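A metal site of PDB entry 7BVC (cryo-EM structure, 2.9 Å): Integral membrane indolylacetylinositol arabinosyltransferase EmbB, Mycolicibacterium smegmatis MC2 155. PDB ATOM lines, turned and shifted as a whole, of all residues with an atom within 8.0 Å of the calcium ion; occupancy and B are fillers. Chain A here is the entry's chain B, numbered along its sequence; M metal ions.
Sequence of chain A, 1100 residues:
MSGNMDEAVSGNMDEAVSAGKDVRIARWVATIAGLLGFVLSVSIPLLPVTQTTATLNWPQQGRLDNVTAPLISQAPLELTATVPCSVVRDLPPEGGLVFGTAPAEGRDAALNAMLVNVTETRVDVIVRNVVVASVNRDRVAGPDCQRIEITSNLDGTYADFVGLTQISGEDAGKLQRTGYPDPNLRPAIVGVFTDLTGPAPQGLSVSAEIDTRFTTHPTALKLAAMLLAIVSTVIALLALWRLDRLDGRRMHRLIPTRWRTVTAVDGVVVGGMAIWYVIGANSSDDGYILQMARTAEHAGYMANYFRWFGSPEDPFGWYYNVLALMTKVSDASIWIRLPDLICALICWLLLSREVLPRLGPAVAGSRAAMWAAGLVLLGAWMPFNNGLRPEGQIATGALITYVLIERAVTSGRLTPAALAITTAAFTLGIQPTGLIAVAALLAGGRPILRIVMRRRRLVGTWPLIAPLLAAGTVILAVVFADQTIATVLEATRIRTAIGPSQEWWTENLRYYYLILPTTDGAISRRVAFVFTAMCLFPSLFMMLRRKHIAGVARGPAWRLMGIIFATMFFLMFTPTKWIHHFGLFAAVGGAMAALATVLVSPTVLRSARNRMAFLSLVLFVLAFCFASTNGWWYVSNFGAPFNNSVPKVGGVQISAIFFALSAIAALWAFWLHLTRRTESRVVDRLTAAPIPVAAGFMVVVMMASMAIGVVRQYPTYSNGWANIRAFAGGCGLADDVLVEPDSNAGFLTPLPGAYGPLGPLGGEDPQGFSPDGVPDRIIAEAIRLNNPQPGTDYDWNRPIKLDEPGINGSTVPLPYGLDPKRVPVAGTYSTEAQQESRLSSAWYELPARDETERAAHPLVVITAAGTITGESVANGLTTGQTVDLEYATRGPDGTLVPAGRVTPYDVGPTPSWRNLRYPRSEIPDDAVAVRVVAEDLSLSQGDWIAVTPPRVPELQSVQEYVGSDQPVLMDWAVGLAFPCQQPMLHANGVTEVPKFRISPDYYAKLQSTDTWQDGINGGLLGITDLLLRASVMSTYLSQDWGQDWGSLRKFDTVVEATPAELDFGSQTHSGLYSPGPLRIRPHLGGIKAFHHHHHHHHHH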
ATOM      1  N   GLY A 768     -22.434  12.117 -12.876  1.00  0.00           N
ATOM      2  CA  GLY A 768     -21.922  11.334 -13.988  1.00  0.00           C
ATOM      3  C   GLY A 768     -21.665  12.132 -15.253  1.00  0.00           C
ATOM      4  O   GLY A 768     -21.908  11.640 -16.357  1.00  0.00           O
ATOM      5  N   THR A 828     -22.849  13.211 -20.756  1.00  0.00           N
ATOM      6  CA  THR A 828     -23.181  11.987 -20.043  1.00  0.00           C
ATOM      7  C   THR A 828     -22.719  10.727 -20.770  1.00  0.00           C
ATOM      8  O   THR A 828     -22.544   9.690 -20.116  1.00  0.00           O
ATOM      9  CB  THR A 828     -24.707  11.919 -19.819  1.00  0.00           C
ATOM     10  OG1 THR A 828     -25.146  13.143 -19.230  1.00  0.00           O
ATOM     11  CG2 THR A 828     -25.076  10.778 -18.900  1.00  0.00           C
ATOM     12  N   TYR A 829     -22.485  10.797 -22.076  1.00  0.00           N
ATOM     13  CA  TYR A 829     -22.130   9.612 -22.851  1.00  0.00           C
ATOM     14  C   TYR A 829     -20.855   8.985 -22.327  1.00  0.00           C
ATOM     15  O   TYR A 829     -19.902   9.673 -21.939  1.00  0.00           O
ATOM     16  CB  TYR A 829     -21.974   9.986 -24.325  1.00  0.00           C
ATOM     17  CG  TYR A 829     -21.572   8.848 -25.236  1.00  0.00           C
ATOM     18  CD1 TYR A 829     -22.511   7.948 -25.700  1.00  0.00           C
ATOM     19  CD2 TYR A 829     -20.246   8.679 -25.619  1.00  0.00           C
ATOM     20  CE1 TYR A 829     -22.152   6.902 -26.539  1.00  0.00           C
ATOM     21  CE2 TYR A 829     -19.880   7.648 -26.453  1.00  0.00           C
ATOM     22  CZ  TYR A 829     -20.827   6.759 -26.902  1.00  0.00           C
ATOM     23  OH  TYR A 829     -20.462   5.727 -27.736  1.00  0.00           O
ATOM     24  N   SER A 830     -20.823   7.653 -22.323  1.00  0.00           N
ATOM     25  CA  SER A 830     -19.688   6.878 -21.845  1.00  0.00           C
ATOM     26  C   SER A 830     -19.672   5.550 -22.571  1.00  0.00           C
ATOM     27  O   SER A 830     -20.689   5.110 -23.118  1.00  0.00           O
ATOM     28  CB  SER A 830     -19.740   6.682 -20.327  1.00  0.00           C
ATOM     29  OG  SER A 830     -18.873   5.633 -19.920  1.00  0.00           O
ATOM     30  N   ALA A 833     -18.975   2.180 -18.660  1.00  0.00           N
ATOM     31  CA  ALA A 833     -19.897   1.823 -17.591  1.00  0.00           C
ATOM     32  C   ALA A 833     -20.995   2.863 -17.496  1.00  0.00           C
ATOM     33  O   ALA A 833     -20.710   4.060 -17.387  1.00  0.00           O
ATOM     34  CB  ALA A 833     -19.157   1.695 -16.244  1.00  0.00           C
ATOM     35  N   GLN A 834     -22.236   2.406 -17.532  1.00  0.00           N
ATOM     36  CA  GLN A 834     -23.387   3.305 -17.482  1.00  0.00           C
ATOM     37  C   GLN A 834     -23.697   3.712 -16.050  1.00  0.00           C
ATOM     38  O   GLN A 834     -23.298   3.056 -15.086  1.00  0.00           O
ATOM     39  CB  GLN A 834     -24.596   2.659 -18.139  1.00  0.00           C
ATOM     40  CG  GLN A 834     -24.293   2.092 -19.520  1.00  0.00           C
ATOM     41  CD  GLN A 834     -23.607   3.097 -20.420  1.00  0.00           C
ATOM     42  OE1 GLN A 834     -23.998   4.274 -20.473  1.00  0.00           O
ATOM     43  NE2 GLN A 834     -22.587   2.650 -21.129  1.00  0.00           N
ATOM     44  N   GLN A 835     -24.434   4.807 -15.910  1.00  0.00           N
ATOM     45  CA  GLN A 835     -24.648   5.421 -14.614  1.00  0.00           C
ATOM     46  C   GLN A 835     -25.829   6.369 -14.701  1.00  0.00           C
ATOM     47  O   GLN A 835     -26.252   6.763 -15.791  1.00  0.00           O
ATOM     48  CB  GLN A 835     -23.384   6.173 -14.147  1.00  0.00           C
ATOM     49  CG  GLN A 835     -23.319   6.478 -12.664  1.00  0.00           C
ATOM     50  CD  GLN A 835     -22.030   7.165 -12.285  1.00  0.00           C
ATOM     51  OE1 GLN A 835     -21.251   7.566 -13.149  1.00  0.00           O
ATOM     52  NE2 GLN A 835     -21.795   7.313 -10.987  1.00  0.00           N
ATOM     53  N   GLU A 836     -26.355   6.730 -13.532  1.00  0.00           N
ATOM     54  CA  GLU A 836     -27.373   7.766 -13.418  1.00  0.00           C
ATOM     55  C   GLU A 836     -26.662   9.088 -13.158  1.00  0.00           C
ATOM     56  O   GLU A 836     -25.864   9.204 -12.231  1.00  0.00           O
ATOM     57  CB  GLU A 836     -28.346   7.456 -12.276  1.00  0.00           C
ATOM     58  CG  GLU A 836     -29.330   6.334 -12.592  1.00  0.00           C
ATOM     59  CD  GLU A 836     -30.352   6.152 -11.493  1.00  0.00           C
ATOM     60  OE1 GLU A 836     -29.958   6.131 -10.308  1.00  0.00           O
ATOM     61  OE2 GLU A 836     -31.556   6.049 -11.810  1.00  0.00           O
ATOM     62  N   SER A 837     -26.958  10.078 -13.992  1.00  0.00           N
ATOM     63  CA  SER A 837     -26.212  11.332 -14.006  1.00  0.00           C
ATOM     64  C   SER A 837     -27.101  12.483 -13.553  1.00  0.00           C
ATOM     65  O   SER A 837     -28.286  12.543 -13.876  1.00  0.00           O
ATOM     66  CB  SER A 837     -25.679  11.616 -15.411  1.00  0.00           C
ATOM     67  OG  SER A 837     -24.540  10.818 -15.698  1.00  0.00           O
ATOM     68  N   THR A 867     -30.615  13.355 -26.159  1.00  0.00           N
ATOM     69  CA  THR A 867     -31.959  12.816 -26.313  1.00  0.00           C
ATOM     70  C   THR A 867     -32.943  13.621 -25.476  1.00  0.00           C
ATOM     71  O   THR A 867     -33.801  13.082 -24.769  1.00  0.00           O
ATOM     72  CB  THR A 867     -31.971  11.319 -25.985  1.00  0.00           C
ATOM     73  OG1 THR A 867     -33.251  10.757 -26.318  1.00  0.00           O
ATOM     74  CG2 THR A 867     -31.627  11.059 -24.517  1.00  0.00           C
ATOM     75  N   GLN A 881     -34.502  12.078 -21.807  1.00  0.00           N
ATOM     76  CA  GLN A 881     -33.857  12.657 -20.634  1.00  0.00           C
ATOM     77  C   GLN A 881     -34.099  14.164 -20.585  1.00  0.00           C
ATOM     78  O   GLN A 881     -34.471  14.786 -21.575  1.00  0.00           O
ATOM     79  CB  GLN A 881     -32.368  12.330 -20.640  1.00  0.00           C
ATOM     80  CG  GLN A 881     -32.066  10.871 -20.927  1.00  0.00           C
ATOM     81  CD  GLN A 881     -32.933   9.921 -20.127  1.00  0.00           C
ATOM     82  OE1 GLN A 881     -33.056  10.048 -18.913  1.00  0.00           O
ATOM     83  NE2 GLN A 881     -33.552   8.966 -20.815  1.00  0.00           N
ATOM     84  N   ASP A 936     -30.143  12.399 -16.645  1.00  0.00           N
ATOM     85  CA  ASP A 936     -30.178  11.277 -17.572  1.00  0.00           C
ATOM     86  C   ASP A 936     -30.258   9.993 -16.743  1.00  0.00           C
ATOM     87  O   ASP A 936     -29.300   9.627 -16.072  1.00  0.00           O
ATOM     88  CB  ASP A 936     -28.939  11.268 -18.473  1.00  0.00           C
ATOM     89  CG  ASP A 936     -28.708   9.917 -19.132  1.00  0.00           C
ATOM     90  OD1 ASP A 936     -29.262   9.690 -20.225  1.00  0.00           O
ATOM     91  OD2 ASP A 936     -27.953   9.096 -18.564  1.00  0.00           O
ATOM     92  N   LEU A 937     -31.415   9.328 -16.792  1.00  0.00           N
ATOM     93  CA  LEU A 937     -31.684   8.170 -15.943  1.00  0.00           C
ATOM     94  C   LEU A 937     -31.780   6.866 -16.721  1.00  0.00           C
ATOM     95  O   LEU A 937     -32.299   5.879 -16.184  1.00  0.00           O
ATOM     96  CB  LEU A 937     -32.958   8.402 -15.138  1.00  0.00           C
ATOM     97  CG  LEU A 937     -32.975   9.599 -14.187  1.00  0.00           C
ATOM     98  CD1 LEU A 937     -34.293   9.658 -13.437  1.00  0.00           C
ATOM     99  CD2 LEU A 937     -31.797   9.529 -13.225  1.00  0.00           C
ATOM    100  N   SER A 938     -31.322   6.835 -17.964  1.00  0.00           N
ATOM    101  CA  SER A 938     -31.347   5.619 -18.772  1.00  0.00           C
ATOM    102  C   SER A 938     -29.957   5.007 -18.832  1.00  0.00           C
ATOM    103  O   SER A 938     -28.976   5.729 -19.061  1.00  0.00           O
ATOM    104  CB  SER A 938     -31.854   5.925 -20.185  1.00  0.00           C
ATOM    105  OG  SER A 938     -32.075   4.731 -20.910  1.00  0.00           O
ATOM    106  N   LEU A 939     -29.873   3.699 -18.611  1.00  0.00           N
ATOM    107  CA  LEU A 939     -28.608   2.994 -18.667  1.00  0.00           C
ATOM    108  C   LEU A 939     -28.284   2.445 -20.050  1.00  0.00           C
ATOM    109  O   LEU A 939     -27.303   1.719 -20.203  1.00  0.00           O
ATOM    110  CB  LEU A 939     -28.588   1.848 -17.655  1.00  0.00           C
ATOM    111  CG  LEU A 939     -28.661   2.172 -16.167  1.00  0.00           C
ATOM    112  CD1 LEU A 939     -28.503   0.890 -15.374  1.00  0.00           C
ATOM    113  CD2 LEU A 939     -27.607   3.189 -15.786  1.00  0.00           C
ATOM    114  N   SER A 940     -29.091   2.764 -21.058  1.00  0.00           N
ATOM    115  CA  SER A 940     -28.733   2.399 -22.412  1.00  0.00           C
ATOM    116  C   SER A 940     -27.577   3.275 -22.887  1.00  0.00           C
ATOM    117  O   SER A 940     -27.374   4.390 -22.414  1.00  0.00           O
ATOM    118  CB  SER A 940     -29.930   2.550 -23.352  1.00  0.00           C
ATOM    119  OG  SER A 940     -29.511   2.549 -24.708  1.00  0.00           O
ATOM    120  N   GLN A 941     -26.809   2.739 -23.844  1.00  0.00           N
ATOM    121  CA  GLN A 941     -25.641   3.472 -24.311  1.00  0.00           C
ATOM    122  C   GLN A 941     -26.028   4.581 -25.287  1.00  0.00           C
ATOM    123  O   GLN A 941     -25.320   5.585 -25.376  1.00  0.00           O
ATOM    124  CB  GLN A 941     -24.645   2.517 -24.968  1.00  0.00           C
ATOM    125  CG  GLN A 941     -23.235   3.075 -25.057  1.00  0.00           C
ATOM    126  CD  GLN A 941     -22.291   2.166 -25.807  1.00  0.00           C
ATOM    127  OE1 GLN A 941     -22.709   1.185 -26.419  1.00  0.00           O
ATOM    128  NE2 GLN A 941     -20.996   2.486 -25.759  1.00  0.00           N
ATOM    129  N   GLY A 942     -27.129   4.423 -26.003  1.00  0.00           N
ATOM    130  CA  GLY A 942     -27.566   5.431 -26.944  1.00  0.00           C
ATOM    131  C   GLY A 942     -28.523   6.443 -26.336  1.00  0.00           C
ATOM    132  O   GLY A 942     -29.264   7.106 -27.064  1.00  0.00           O
ATOM    133  N   ASP A 943     -28.511   6.571 -25.007  1.00  0.00           N
ATOM    134  CA  ASP A 943     -29.334   7.541 -24.294  1.00  0.00           C
ATOM    135  C   ASP A 943     -28.417   8.401 -23.439  1.00  0.00           C
ATOM    136  O   ASP A 943     -27.971   7.977 -22.368  1.00  0.00           O
ATOM    137  CB  ASP A 943     -30.405   6.856 -23.452  1.00  0.00           C
ATOM    138  CG  ASP A 943     -31.480   6.191 -24.298  1.00  0.00           C
ATOM    139  OD1 ASP A 943     -31.725   6.657 -25.429  1.00  0.00           O
ATOM    140  OD2 ASP A 943     -32.078   5.199 -23.828  1.00  0.00           O
ATOM    141  N   TRP A 944     -28.128   9.610 -23.915  1.00  0.00           N
ATOM    142  CA  TRP A 944     -27.172  10.504 -23.272  1.00  0.00           C
ATOM    143  C   TRP A 944     -27.628  11.939 -23.505  1.00  0.00           C
ATOM    144  O   TRP A 944     -28.514  12.204 -24.307  1.00  0.00           O
ATOM    145  CB  TRP A 944     -25.760  10.281 -23.802  1.00  0.00           C
ATOM    146  CG  TRP A 944     -25.671  10.472 -25.280  1.00  0.00           C
ATOM    147  CD1 TRP A 944     -25.992   9.558 -26.237  1.00  0.00           C
ATOM    148  CD2 TRP A 944     -25.257  11.648 -25.968  1.00  0.00           C
ATOM    149  NE1 TRP A 944     -25.803  10.090 -27.484  1.00  0.00           N
ATOM    150  CE2 TRP A 944     -25.349  11.377 -27.353  1.00  0.00           C
ATOM    151  CE3 TRP A 944     -24.817  12.913 -25.564  1.00  0.00           C
ATOM    152  CZ2 TRP A 944     -25.014  12.324 -28.318  1.00  0.00           C
ATOM    153  CZ3 TRP A 944     -24.495  13.842 -26.523  1.00  0.00           C
ATOM    154  CH2 TRP A 944     -24.596  13.552 -27.884  1.00  0.00           C
ATOM    155  N   ILE A 945     -26.987  12.872 -22.789  1.00  0.00           N
ATOM    156  CA  ILE A 945     -27.254  14.294 -22.949  1.00  0.00           C
ATOM    157  C   ILE A 945     -25.929  15.053 -22.854  1.00  0.00           C
ATOM    158  O   ILE A 945     -24.892  14.495 -22.501  1.00  0.00           O
ATOM    159  CB  ILE A 945     -28.245  14.830 -21.895  1.00  0.00           C
ATOM    160  CG1 ILE A 945     -27.736  14.589 -20.476  1.00  0.00           C
ATOM    161  CG2 ILE A 945     -29.624  14.210 -22.072  1.00  0.00           C
ATOM    162  CD1 ILE A 945     -28.763  14.864 -19.404  1.00  0.00           C
HETATM  163 CA    CA M   1     -27.042   7.025 -20.043  1.00  0.00          CA
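The calcium ion is bound by the backbone carbonyl oxygen of Ser 938 (2.5 Å), the backbone carbonyl oxygen of Asp 943 (2.7 Å) and the side-chain carboxylate of Asp 936 (2.7 Å).
The backbone carbonyl oxygen of Asp 936 sits at hydrogen-bond distance from the backbone NH of Ser 837.
OG of Ser 940 lies within hydrogen-bond range of N of Gly 942 (3.3 Å).
Ser 940 touches the calcium ion.
The nearest printed residue that does not touch the calcium ion is Gln 834 (4.1 Å).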
